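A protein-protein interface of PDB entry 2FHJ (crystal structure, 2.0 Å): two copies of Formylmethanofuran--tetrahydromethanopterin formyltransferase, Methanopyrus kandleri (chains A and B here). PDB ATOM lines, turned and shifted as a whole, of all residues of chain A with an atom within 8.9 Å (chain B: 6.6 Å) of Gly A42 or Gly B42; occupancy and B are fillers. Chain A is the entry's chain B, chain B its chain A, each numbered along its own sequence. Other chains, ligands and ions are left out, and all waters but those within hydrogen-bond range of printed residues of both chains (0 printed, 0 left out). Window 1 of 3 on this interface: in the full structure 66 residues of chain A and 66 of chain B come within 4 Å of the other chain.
OE1 of Glu A39 sits at hydrogen-bond distance from N of Gly B44 (2.7 Å).
The backbone carbonyl oxygen of Glu A39 sits at hydrogen-bond distance from the backbone NH of Phe B43.
The backbone carbonyl oxygen (O) of Glu B39 sits at hydrogen-bond distance from the backbone NH (N) of Phe A43, at 2.7 Å.
The side-chain carboxylate of Glu B39 sits at hydrogen-bond distance from the backbone NH of Gly A44, 2.7 Å away.
The side-chain hydroxyl (OG1) of Thr A41 sits at hydrogen-bond distance from the backbone carbonyl oxygen (O) of Val A37.
The guanidinium group (NH2) of Arg B92 is in hydrogen-bond range of the backbone carbonyl oxygen (O) of Gly B42, 2.6 Å away.
The backbone carbonyl oxygen (O) of Gly A44 sits at hydrogen-bond distance from the backbone NH (N) of Ala A54 (2.9 Å).
N of Ala B54 sits at hydrogen-bond distance from O of Gly B44, 2.9 Å away.
O of Val B37 lies within hydrogen-bond range of OG1 of Thr B41, at 2.9 Å.
O of Phe A43 sits at hydrogen-bond distance from NH2 of Arg A92, 3.5 Å away.
Among the printed residues, pairs that only touch across the chains: Glu A39 with Thr B45, Gly A42 with Phe B43, Thr A45 with Glu B39, Phe A43 with Gly B42, Gly A42 with Glu B39, Glu A39 with Gly B42, Gln A88 with Phe B43, Arg A92 with Phe B43, Phe A43 with Arg B92, Thr A41 with Glu B39, Gly A42 with Gly B42, Glu A39 with Thr B41, Phe A43 with Pro B51, Pro A51 with Phe B43, Cys A96 with Phe B43, Phe A43 with Phe B43 and Phe A43 with Cys B96.
Gly A42 touches just these residues of chain B: Glu B39, Gly B42 and Phe B43.
Gly B42 touches three residues of chain A.
Thr B41 touches just one residue of chain A: Glu A39.
Of the printed residues of chain B, Glu A39 touches Thr B41, Gly B42, Phe B43, Gly B44 and Thr B45.
Printed residues of chain A within 4 Å of Pro B51: Phe A43 (3.9 Å).
The nearest printed residue of chain A that does not touch Phe B43 is Ala A40 (4.9 Å).
Of the 15 printed residues of chain B, 9 touch a printed residue of chain A.
Of the 27 printed residues of chain A, 10 touch a printed residue of chain B.
Along chain A the printed residues that touch a printed residue of chain B span positions 39 to 96.
Among the printed residues, 21 pairs touch across the chains.
Among the printed residues, no Asp or Glu carboxylate lies within 4 Å of a Lys or Arg side-chain nitrogen of the other chain.
Glu A39 touches Gly B44, and with the chains exchanged Gly A44 touches Glu B39.
Gly B42 touches its own counterpart, Gly A42.
Phe A43 touches Pro B51, and with the chains exchanged Pro A51 touches Phe B43.
Phe A43 touches Cys B96, and with the chains exchanged Cys A96 touches Phe B43.
Positions printed for both chains: 37, 38, 39, 40, 41, 42, 43, 44, 45, 51, 52, 54, 55, 92 and 96.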
ATOM      1  N   MET A  34       0.310  34.097 -21.212  1.00  0.00           N
ATOM      2  CA  MET A  34       1.739  33.959 -20.966  1.00  0.00           C
ATOM      3  C   MET A  34       2.120  32.885 -19.950  1.00  0.00           C
ATOM      4  O   MET A  34       3.194  32.307 -20.045  1.00  0.00           O
ATOM      5  CB  MET A  34       2.326  35.307 -20.540  1.00  0.00           C
ATOM      6  CG  MET A  34       2.530  36.288 -21.698  1.00  0.00           C
ATOM      7  SD  MET A  34       3.582  35.669 -23.039  1.00  0.00           S
ATOM      8  CE  MET A  34       4.917  34.901 -22.113  1.00  0.00           C
ATOM      9  N   ILE A  35       1.268  32.645 -18.960  1.00  0.00           N
ATOM     10  CA  ILE A  35       1.466  31.547 -18.001  1.00  0.00           C
ATOM     11  C   ILE A  35       1.514  30.199 -18.726  1.00  0.00           C
ATOM     12  O   ILE A  35       2.337  29.337 -18.403  1.00  0.00           O
ATOM     13  CB  ILE A  35       0.307  31.513 -16.949  1.00  0.00           C
ATOM     14  CG1 ILE A  35       0.402  32.711 -15.994  1.00  0.00           C
ATOM     15  CG2 ILE A  35       0.288  30.194 -16.174  1.00  0.00           C
ATOM     16  CD1 ILE A  35       1.481  32.603 -14.962  1.00  0.00           C
ATOM     17  N   ALA A  36       0.607  30.027 -19.682  1.00  0.00           N
ATOM     18  CA  ALA A  36       0.508  28.796 -20.457  1.00  0.00           C
ATOM     19  C   ALA A  36       1.659  28.667 -21.457  1.00  0.00           C
ATOM     20  O   ALA A  36       2.209  27.586 -21.657  1.00  0.00           O
ATOM     21  CB  ALA A  36      -0.824  28.766 -21.178  1.00  0.00           C
ATOM     22  N   VAL A  37       1.995  29.784 -22.080  1.00  0.00           N
ATOM     23  CA  VAL A  37       3.058  29.864 -23.076  1.00  0.00           C
ATOM     24  C   VAL A  37       4.419  29.490 -22.513  1.00  0.00           C
ATOM     25  O   VAL A  37       5.105  28.639 -23.063  1.00  0.00           O
ATOM     26  CB  VAL A  37       3.142  31.298 -23.642  1.00  0.00           C
ATOM     27  CG1 VAL A  37       4.447  31.514 -24.372  1.00  0.00           C
ATOM     28  CG2 VAL A  37       1.961  31.563 -24.562  1.00  0.00           C
ATOM     29  N   LYS A  38       4.807  30.148 -21.424  1.00  0.00           N
ATOM     30  CA  LYS A  38       6.065  29.872 -20.755  1.00  0.00           C
ATOM     31  C   LYS A  38       6.212  28.421 -20.331  1.00  0.00           C
ATOM     32  O   LYS A  38       7.288  27.825 -20.478  1.00  0.00           O
ATOM     33  CB  LYS A  38       6.185  30.746 -19.520  1.00  0.00           C
ATOM     34  CG  LYS A  38       6.323  32.215 -19.837  1.00  0.00           C
ATOM     35  CD  LYS A  38       7.374  32.426 -20.925  1.00  0.00           C
ATOM     36  CE  LYS A  38       8.301  33.591 -20.667  1.00  0.00           C
ATOM     37  NZ  LYS A  38       9.484  33.391 -21.580  1.00  0.00           N
ATOM     38  N   GLU A  39       5.145  27.864 -19.768  1.00  0.00           N
ATOM     39  CA  GLU A  39       5.192  26.477 -19.346  1.00  0.00           C
ATOM     40  C   GLU A  39       5.365  25.599 -20.573  1.00  0.00           C
ATOM     41  O   GLU A  39       6.180  24.673 -20.568  1.00  0.00           O
ATOM     42  CB  GLU A  39       3.934  26.106 -18.561  1.00  0.00           C
ATOM     43  CG  GLU A  39       3.950  24.683 -18.001  1.00  0.00           C
ATOM     44  CD  GLU A  39       5.102  24.416 -17.040  1.00  0.00           C
ATOM     45  OE1 GLU A  39       5.666  23.290 -17.046  1.00  0.00           O
ATOM     46  OE2 GLU A  39       5.441  25.321 -16.251  1.00  0.00           O
ATOM     47  N   ALA A  40       4.614  25.920 -21.622  1.00  0.00           N
ATOM     48  CA  ALA A  40       4.549  25.082 -22.818  1.00  0.00           C
ATOM     49  C   ALA A  40       5.818  25.156 -23.669  1.00  0.00           C
ATOM     50  O   ALA A  40       6.210  24.166 -24.308  1.00  0.00           O
ATOM     51  CB  ALA A  40       3.330  25.472 -23.656  1.00  0.00           C
ATOM     52  N   THR A  41       6.455  26.328 -23.683  1.00  0.00           N
ATOM     53  CA  THR A  41       7.667  26.530 -24.458  1.00  0.00           C
ATOM     54  C   THR A  41       8.922  26.396 -23.611  1.00  0.00           C
ATOM     55  O   THR A  41      10.022  26.575 -24.129  1.00  0.00           O
ATOM     56  CB  THR A  41       7.698  27.903 -25.138  1.00  0.00           C
ATOM     57  OG1 THR A  41       7.706  28.928 -24.140  1.00  0.00           O
ATOM     58  CG2 THR A  41       6.521  28.092 -26.059  1.00  0.00           C
ATOM     59  N   GLY A  42       8.782  26.080 -22.324  1.00  0.00           N
ATOM     60  CA  GLY A  42       9.947  25.857 -21.461  1.00  0.00           C
ATOM     61  C   GLY A  42      10.602  24.497 -21.684  1.00  0.00           C
ATOM     62  O   GLY A  42      10.053  23.664 -22.394  1.00  0.00           O
ATOM     63  N   PHE A  43      11.767  24.273 -21.069  1.00  0.00           N
ATOM     64  CA  PHE A  43      12.599  23.084 -21.341  1.00  0.00           C
ATOM     65  C   PHE A  43      12.659  22.774 -22.847  1.00  0.00           C
ATOM     66  O   PHE A  43      12.420  21.638 -23.282  1.00  0.00           O
ATOM     67  CB  PHE A  43      12.081  21.880 -20.534  1.00  0.00           C
ATOM     68  CG  PHE A  43      12.960  20.638 -20.596  1.00  0.00           C
ATOM     69  CD1 PHE A  43      14.346  20.726 -20.715  1.00  0.00           C
ATOM     70  CD2 PHE A  43      12.381  19.374 -20.491  1.00  0.00           C
ATOM     71  CE1 PHE A  43      15.139  19.576 -20.754  1.00  0.00           C
ATOM     72  CE2 PHE A  43      13.170  18.210 -20.526  1.00  0.00           C
ATOM     73  CZ  PHE A  43      14.548  18.319 -20.651  1.00  0.00           C
ATOM     74  N   GLY A  44      12.993  23.791 -23.633  1.00  0.00           N
ATOM     75  CA  GLY A  44      12.906  23.697 -25.093  1.00  0.00           C
ATOM     76  C   GLY A  44      13.823  24.685 -25.784  1.00  0.00           C
ATOM     77  O   GLY A  44      13.364  25.583 -26.503  1.00  0.00           O
ATOM     78  N   THR A  45      15.117  24.560 -25.506  1.00  0.00           N
ATOM     79  CA  THR A  45      16.136  25.472 -26.040  1.00  0.00           C
ATOM     80  C   THR A  45      16.849  24.849 -27.223  1.00  0.00           C
ATOM     81  O   THR A  45      17.169  25.542 -28.183  1.00  0.00           O
ATOM     82  CB  THR A  45      17.208  25.872 -24.984  1.00  0.00           C
ATOM     83  OG1 THR A  45      17.922  24.728 -24.532  1.00  0.00           O
ATOM     84  CG2 THR A  45      16.587  26.554 -23.781  1.00  0.00           C
ATOM     85  N   SER A  46      17.065  23.540 -27.146  1.00  0.00           N
ATOM     86  CA  SER A  46      17.873  22.815 -28.113  1.00  0.00           C
ATOM     87  C   SER A  46      17.601  21.303 -28.066  1.00  0.00           C
ATOM     88  O   SER A  46      17.531  20.712 -26.993  1.00  0.00           O
ATOM     89  CB  SER A  46      19.348  23.075 -27.830  1.00  0.00           C
ATOM     90  OG  SER A  46      20.132  21.921 -28.077  1.00  0.00           O
ATOM     91  N   CYS A  50      17.137  18.714 -25.039  1.00  0.00           N
ATOM     92  CA  CYS A  50      15.727  19.003 -24.760  1.00  0.00           C
ATOM     93  C   CYS A  50      14.857  18.203 -25.711  1.00  0.00           C
ATOM     94  O   CYS A  50      15.316  17.782 -26.774  1.00  0.00           O
ATOM     95  CB  CYS A  50      15.396  20.477 -24.900  1.00  0.00           C
ATOM     96  SG  CYS A  50      16.390  21.494 -23.869  1.00  0.00           S
ATOM     97  N   PRO A  51      13.597  17.975 -25.328  1.00  0.00           N
ATOM     98  CA  PRO A  51      12.679  17.281 -26.196  1.00  0.00           C
ATOM     99  C   PRO A  51      12.230  18.091 -27.413  1.00  0.00           C
ATOM    100  O   PRO A  51      11.759  17.498 -28.372  1.00  0.00           O
ATOM    101  CB  PRO A  51      11.497  16.979 -25.274  1.00  0.00           C
ATOM    102  CG  PRO A  51      12.003  17.228 -23.886  1.00  0.00           C
ATOM    103  CD  PRO A  51      12.963  18.318 -24.045  1.00  0.00           C
ATOM    104  N   ALA A  52      12.362  19.415 -27.381  1.00  0.00           N
ATOM    105  CA  ALA A  52      12.045  20.240 -28.546  1.00  0.00           C
ATOM    106  C   ALA A  52      12.760  21.580 -28.523  1.00  0.00           C
ATOM    107  O   ALA A  52      13.509  21.885 -27.594  1.00  0.00           O
ATOM    108  CB  ALA A  52      10.559  20.467 -28.640  1.00  0.00           C
ATOM    109  N   GLU A  53      12.533  22.367 -29.570  1.00  0.00           N
ATOM    110  CA  GLU A  53      12.952  23.751 -29.600  1.00  0.00           C
ATOM    111  C   GLU A  53      11.703  24.605 -29.724  1.00  0.00           C
ATOM    112  O   GLU A  53      11.008  24.575 -30.737  1.00  0.00           O
ATOM    113  CB  GLU A  53      13.903  23.987 -30.766  1.00  0.00           C
ATOM    114  CG  GLU A  53      15.298  23.462 -30.525  1.00  0.00           C
ATOM    115  CD  GLU A  53      16.170  23.470 -31.776  1.00  0.00           C
ATOM    116  OE1 GLU A  53      15.844  24.212 -32.723  1.00  0.00           O
ATOM    117  OE2 GLU A  53      17.197  22.747 -31.795  1.00  0.00           O
ATOM    118  N   ALA A  54      11.417  25.381 -28.692  1.00  0.00           N
ATOM    119  CA  ALA A  54      10.147  26.080 -28.610  1.00  0.00           C
ATOM    120  C   ALA A  54      10.360  27.499 -28.138  1.00  0.00           C
ATOM    121  O   ALA A  54      11.348  27.802 -27.475  1.00  0.00           O
ATOM    122  CB  ALA A  54       9.220  25.346 -27.657  1.00  0.00           C
ATOM    123  N   GLY A  55       9.427  28.373 -28.462  1.00  0.00           N
ATOM    124  CA  GLY A  55       9.529  29.742 -27.996  1.00  0.00           C
ATOM    125  C   GLY A  55       8.393  30.574 -28.514  1.00  0.00           C
ATOM    126  O   GLY A  55       7.597  30.120 -29.329  1.00  0.00           O
ATOM    127  N   ILE A  56       8.342  31.813 -28.045  1.00  0.00           N
ATOM    128  CA  ILE A  56       7.281  32.708 -28.396  1.00  0.00           C
ATOM    129  C   ILE A  56       7.568  33.324 -29.755  1.00  0.00           C
ATOM    130  O   ILE A  56       8.701  33.744 -30.032  1.00  0.00           O
ATOM    131  CB  ILE A  56       7.141  33.804 -27.336  1.00  0.00           C
ATOM    132  CG1 ILE A  56       6.727  33.157 -26.012  1.00  0.00           C
ATOM    133  CG2 ILE A  56       6.110  34.826 -27.767  1.00  0.00           C
ATOM    134  CD1 ILE A  56       7.006  33.989 -24.794  1.00  0.00           C
ATOM    135  N   ILE A  75       3.124  30.889 -30.390  1.00  0.00           N
ATOM    136  CA  ILE A  75       4.353  30.236 -30.048  1.00  0.00           C
ATOM    137  C   ILE A  75       4.707  29.292 -31.184  1.00  0.00           C
ATOM    138  O   ILE A  75       3.864  28.955 -31.989  1.00  0.00           O
ATOM    139  CB  ILE A  75       4.249  29.412 -28.720  1.00  0.00           C
ATOM    140  CG1 ILE A  75       3.292  28.215 -28.854  1.00  0.00           C
ATOM    141  CG2 ILE A  75       3.824  30.289 -27.569  1.00  0.00           C
ATOM    142  CD1 ILE A  75       3.324  27.301 -27.660  1.00  0.00           C
ATOM    143  N   MET A  76       5.959  28.876 -31.254  1.00  0.00           N
ATOM    144  CA  MET A  76       6.357  27.868 -32.235  1.00  0.00           C
ATOM    145  C   MET A  76       7.106  26.757 -31.539  1.00  0.00           C
ATOM    146  O   MET A  76       7.815  26.995 -30.577  1.00  0.00           O
ATOM    147  CB  MET A  76       7.207  28.498 -33.341  1.00  0.00           C
ATOM    148  CG  MET A  76       6.502  29.624 -34.078  1.00  0.00           C
ATOM    149  SD  MET A  76       7.456  30.465 -35.361  1.00  0.00           S
ATOM    150  CE  MET A  76       7.991  29.018 -36.314  1.00  0.00           C
ATOM    151  N   ILE A  77       6.908  25.541 -32.023  1.00  0.00           N
ATOM    152  CA  ILE A  77       7.575  24.375 -31.521  1.00  0.00           C
ATOM    153  C   ILE A  77       8.154  23.635 -32.729  1.00  0.00           C
ATOM    154  O   ILE A  77       7.470  23.447 -33.728  1.00  0.00           O
ATOM    155  CB  ILE A  77       6.595  23.429 -30.788  1.00  0.00           C
ATOM    156  CG1 ILE A  77       5.837  24.179 -29.680  1.00  0.00           C
ATOM    157  CG2 ILE A  77       7.335  22.201 -30.208  1.00  0.00           C
ATOM    158  CD1 ILE A  77       4.743  23.344 -29.008  1.00  0.00           C
ATOM    159  N   GLN A  88       5.471  16.051 -29.277  1.00  0.00           N
ATOM    160  CA  GLN A  88       5.721  17.242 -28.470  1.00  0.00           C
ATOM    161  C   GLN A  88       4.574  18.238 -28.511  1.00  0.00           C
ATOM    162  O   GLN A  88       4.369  18.996 -27.563  1.00  0.00           O
ATOM    163  CB  GLN A  88       7.031  17.909 -28.894  1.00  0.00           C
ATOM    164  CG  GLN A  88       8.270  17.136 -28.482  1.00  0.00           C
ATOM    165  CD  GLN A  88       8.455  17.097 -26.988  1.00  0.00           C
ATOM    166  OE1 GLN A  88       8.471  18.135 -26.342  1.00  0.00           O
ATOM    167  NE2 GLN A  88       8.600  15.900 -26.427  1.00  0.00           N
ATOM    168  N   ARG A  92       3.002  19.014 -24.822  1.00  0.00           N
ATOM    169  CA  ARG A  92       3.049  20.385 -24.299  1.00  0.00           C
ATOM    170  C   ARG A  92       1.676  21.023 -24.250  1.00  0.00           C
ATOM    171  O   ARG A  92       1.363  21.720 -23.291  1.00  0.00           O
ATOM    172  CB  ARG A  92       4.014  21.231 -25.126  1.00  0.00           C
ATOM    173  CG  ARG A  92       5.452  20.705 -25.055  1.00  0.00           C
ATOM    174  CD  ARG A  92       6.340  21.294 -26.122  1.00  0.00           C
ATOM    175  NE  ARG A  92       7.504  21.856 -25.527  1.00  0.00           N
ATOM    176  CZ  ARG A  92       8.642  21.418 -25.024  1.00  0.00           C
ATOM    177  NH1 ARG A  92       9.427  20.443 -25.457  1.00  0.00           N
ATOM    178  NH2 ARG A  92       9.168  22.334 -24.267  1.00  0.00           N
ATOM    179  N   CYS A  96       0.498  21.347 -20.607  1.00  0.00           N
ATOM    180  CA  CYS A  96       0.820  22.726 -20.212  1.00  0.00           C
ATOM    181  C   CYS A  96      -0.164  23.779 -20.653  1.00  0.00           C
ATOM    182  O   CYS A  96      -0.155  24.897 -20.110  1.00  0.00           O
ATOM    183  CB  CYS A  96       2.182  23.119 -20.760  1.00  0.00           C
ATOM    184  SG  CYS A  96       3.468  21.899 -20.436  1.00  0.00           S
ATOM    185  N   PRO A 199      14.889  30.171 -29.362  1.00  0.00           N
ATOM    186  CA  PRO A 199      14.542  29.193 -28.341  1.00  0.00           C
ATOM    187  C   PRO A 199      15.331  29.231 -27.033  1.00  0.00           C
ATOM    188  O   PRO A 199      14.893  28.607 -26.067  1.00  0.00           O
ATOM    189  CB  PRO A 199      14.745  27.836 -29.053  1.00  0.00           C
ATOM    190  CG  PRO A 199      15.733  28.098 -30.105  1.00  0.00           C
ATOM    191  CD  PRO A 199      15.547  29.546 -30.521  1.00  0.00           C
ATOM    192  N   VAL B  37      15.344  30.121 -14.679  1.00  0.00           N
ATOM    193  CA  VAL B  37      14.404  29.337 -13.874  1.00  0.00           C
ATOM    194  C   VAL B  37      13.201  28.882 -14.678  1.00  0.00           C
ATOM    195  O   VAL B  37      12.880  27.694 -14.724  1.00  0.00           O
ATOM    196  CB  VAL B  37      13.918  30.154 -12.677  1.00  0.00           C
ATOM    197  CG1 VAL B  37      12.676  29.548 -12.069  1.00  0.00           C
ATOM    198  CG2 VAL B  37      15.031  30.269 -11.651  1.00  0.00           C
ATOM    199  N   LYS B  38      12.535  29.830 -15.301  1.00  0.00           N
ATOM    200  CA  LYS B  38      11.390  29.550 -16.152  1.00  0.00           C
ATOM    201  C   LYS B  38      11.673  28.542 -17.256  1.00  0.00           C
ATOM    202  O   LYS B  38      10.874  27.640 -17.519  1.00  0.00           O
ATOM    203  CB  LYS B  38      10.893  30.845 -16.779  1.00  0.00           C
ATOM    204  CG  LYS B  38      10.301  31.823 -15.780  1.00  0.00           C
ATOM    205  CD  LYS B  38       9.356  31.113 -14.821  1.00  0.00           C
ATOM    206  CE  LYS B  38       8.068  31.855 -14.551  1.00  0.00           C
ATOM    207  NZ  LYS B  38       7.081  30.870 -13.983  1.00  0.00           N
ATOM    208  N   GLU B  39      12.793  28.713 -17.923  1.00  0.00           N
ATOM    209  CA  GLU B  39      13.147  27.793 -18.978  1.00  0.00           C
ATOM    210  C   GLU B  39      13.394  26.423 -18.379  1.00  0.00           C
ATOM    211  O   GLU B  39      12.972  25.401 -18.935  1.00  0.00           O
ATOM    212  CB  GLU B  39      14.379  28.303 -19.724  1.00  0.00           C
ATOM    213  CG  GLU B  39      14.768  27.450 -20.918  1.00  0.00           C
ATOM    214  CD  GLU B  39      13.685  27.357 -21.956  1.00  0.00           C
ATOM    215  OE1 GLU B  39      13.479  26.255 -22.526  1.00  0.00           O
ATOM    216  OE2 GLU B  39      13.042  28.384 -22.213  1.00  0.00           O
ATOM    217  N   ALA B  40      14.062  26.404 -17.231  1.00  0.00           N
ATOM    218  CA  ALA B  40      14.503  25.165 -16.617  1.00  0.00           C
ATOM    219  C   ALA B  40      13.367  24.400 -15.971  1.00  0.00           C
ATOM    220  O   ALA B  40      13.404  23.174 -15.939  1.00  0.00           O
ATOM    221  CB  ALA B  40      15.587  25.437 -15.598  1.00  0.00           C
ATOM    222  N   THR B  41      12.373  25.117 -15.442  1.00  0.00           N
ATOM    223  CA  THR B  41      11.244  24.486 -14.773  1.00  0.00           C
ATOM    224  C   THR B  41      10.056  24.324 -15.688  1.00  0.00           C
ATOM    225  O   THR B  41       9.076  23.730 -15.281  1.00  0.00           O
ATOM    226  CB  THR B  41      10.817  25.243 -13.499  1.00  0.00           C
ATOM    227  OG1 THR B  41      10.405  26.567 -13.823  1.00  0.00           O
ATOM    228  CG2 THR B  41      11.948  25.316 -12.512  1.00  0.00           C
ATOM    229  N   GLY B  42      10.141  24.819 -16.923  1.00  0.00           N
ATOM    230  CA  GLY B  42       9.034  24.735 -17.883  1.00  0.00           C
ATOM    231  C   GLY B  42       8.863  23.324 -18.415  1.00  0.00           C
ATOM    232  O   GLY B  42       9.687  22.468 -18.137  1.00  0.00           O
ATOM    233  N   PHE B  43       7.797  23.090 -19.187  1.00  0.00           N
ATOM    234  CA  PHE B  43       7.409  21.729 -19.636  1.00  0.00           C
ATOM    235  C   PHE B  43       7.559  20.667 -18.530  1.00  0.00           C
ATOM    236  O   PHE B  43       8.147  19.600 -18.731  1.00  0.00           O
ATOM    237  CB  PHE B  43       8.203  21.340 -20.893  1.00  0.00           C
ATOM    238  CG  PHE B  43       7.778  20.030 -21.535  1.00  0.00           C
ATOM    239  CD1 PHE B  43       6.449  19.599 -21.514  1.00  0.00           C
ATOM    240  CD2 PHE B  43       8.715  19.249 -22.207  1.00  0.00           C
ATOM    241  CE1 PHE B  43       6.070  18.383 -22.125  1.00  0.00           C
ATOM    242  CE2 PHE B  43       8.338  18.037 -22.831  1.00  0.00           C
ATOM    243  CZ  PHE B  43       7.013  17.616 -22.789  1.00  0.00           C
ATOM    244  N   GLY B  44       7.010  20.972 -17.364  1.00  0.00           N
ATOM    245  CA  GLY B  44       7.248  20.186 -16.164  1.00  0.00           C
ATOM    246  C   GLY B  44       6.127  20.331 -15.161  1.00  0.00           C
ATOM    247  O   GLY B  44       6.346  20.758 -14.028  1.00  0.00           O
ATOM    248  N   THR B  45       4.915  20.009 -15.593  1.00  0.00           N
ATOM    249  CA  THR B  45       3.727  20.143 -14.743  1.00  0.00           C
ATOM    250  C   THR B  45       3.370  18.821 -14.088  1.00  0.00           C
ATOM    251  O   THR B  45       2.913  18.785 -12.944  1.00  0.00           O
ATOM    252  CB  THR B  45       2.497  20.635 -15.543  1.00  0.00           C
ATOM    253  OG1 THR B  45       2.186  19.697 -16.575  1.00  0.00           O
ATOM    254  CG2 THR B  45       2.745  22.006 -16.164  1.00  0.00           C
ATOM    255  N   PRO B  51       8.428  15.315 -18.877  1.00  0.00           N
ATOM    256  CA  PRO B  51       9.609  14.599 -18.398  1.00  0.00           C
ATOM    257  C   PRO B  51       9.890  14.797 -16.906  1.00  0.00           C
ATOM    258  O   PRO B  51      10.641  14.020 -16.335  1.00  0.00           O
ATOM    259  CB  PRO B  51      10.735  15.183 -19.252  1.00  0.00           C
ATOM    260  CG  PRO B  51      10.050  15.928 -20.363  1.00  0.00           C
ATOM    261  CD  PRO B  51       8.805  16.429 -19.764  1.00  0.00           C
ATOM    262  N   ALA B  52       9.314  15.829 -16.282  1.00  0.00           N
ATOM    263  CA  ALA B  52       9.441  16.009 -14.840  1.00  0.00           C
ATOM    264  C   ALA B  52       8.331  16.864 -14.244  1.00  0.00           C
ATOM    265  O   ALA B  52       7.441  17.340 -14.950  1.00  0.00           O
ATOM    266  CB  ALA B  52      10.798  16.617 -14.502  1.00  0.00           C
ATOM    267  N   ALA B  54       8.420  20.257 -12.067  1.00  0.00           N
ATOM    268  CA  ALA B  54       9.386  21.258 -11.667  1.00  0.00           C
ATOM    269  C   ALA B  54       8.704  22.577 -11.384  1.00  0.00           C
ATOM    270  O   ALA B  54       7.628  22.851 -11.902  1.00  0.00           O
ATOM    271  CB  ALA B  54      10.427  21.429 -12.763  1.00  0.00           C
ATOM    272  N   GLY B  55       9.341  23.407 -10.581  1.00  0.00           N
ATOM    273  CA  GLY B  55       8.772  24.707 -10.277  1.00  0.00           C
ATOM    274  C   GLY B  55       9.609  25.486  -9.309  1.00  0.00           C
ATOM    275  O   GLY B  55      10.557  24.983  -8.737  1.00  0.00           O
ATOM    276  N   ARG B  92      18.066  19.766 -17.852  1.00  0.00           N
ATOM    277  CA  ARG B  92      17.541  21.114 -17.612  1.00  0.00           C
ATOM    278  C   ARG B  92      18.621  22.090 -17.169  1.00  0.00           C
ATOM    279  O   ARG B  92      18.609  23.250 -17.572  1.00  0.00           O
ATOM    280  CB  ARG B  92      16.416  21.076 -16.588  1.00  0.00           C
ATOM    281  CG  ARG B  92      15.209  20.298 -17.048  1.00  0.00           C
ATOM    282  CD  ARG B  92      14.262  20.109 -15.898  1.00  0.00           C
ATOM    283  NE  ARG B  92      13.073  19.385 -16.233  1.00  0.00           N
ATOM    284  CZ  ARG B  92      11.983  19.636 -16.935  1.00  0.00           C
ATOM    285  NH1 ARG B  92      11.289  18.547 -17.173  1.00  0.00           N
ATOM    286  NH2 ARG B  92      11.429  20.801 -17.179  1.00  0.00           N
ATOM    287  N   CYS B  96      19.328  24.545 -20.079  1.00  0.00           N
ATOM    288  CA  CYS B  96      18.543  25.745 -19.759  1.00  0.00           C
ATOM    289  C   CYS B  96      19.187  26.701 -18.766  1.00  0.00           C
ATOM    290  O   CYS B  96      18.791  27.879 -18.705  1.00  0.00           O
ATOM    291  CB  CYS B  96      17.176  25.348 -19.198  1.00  0.00           C
ATOM    292  SG  CYS B  96      16.296  24.132 -20.178  1.00  0.00           S
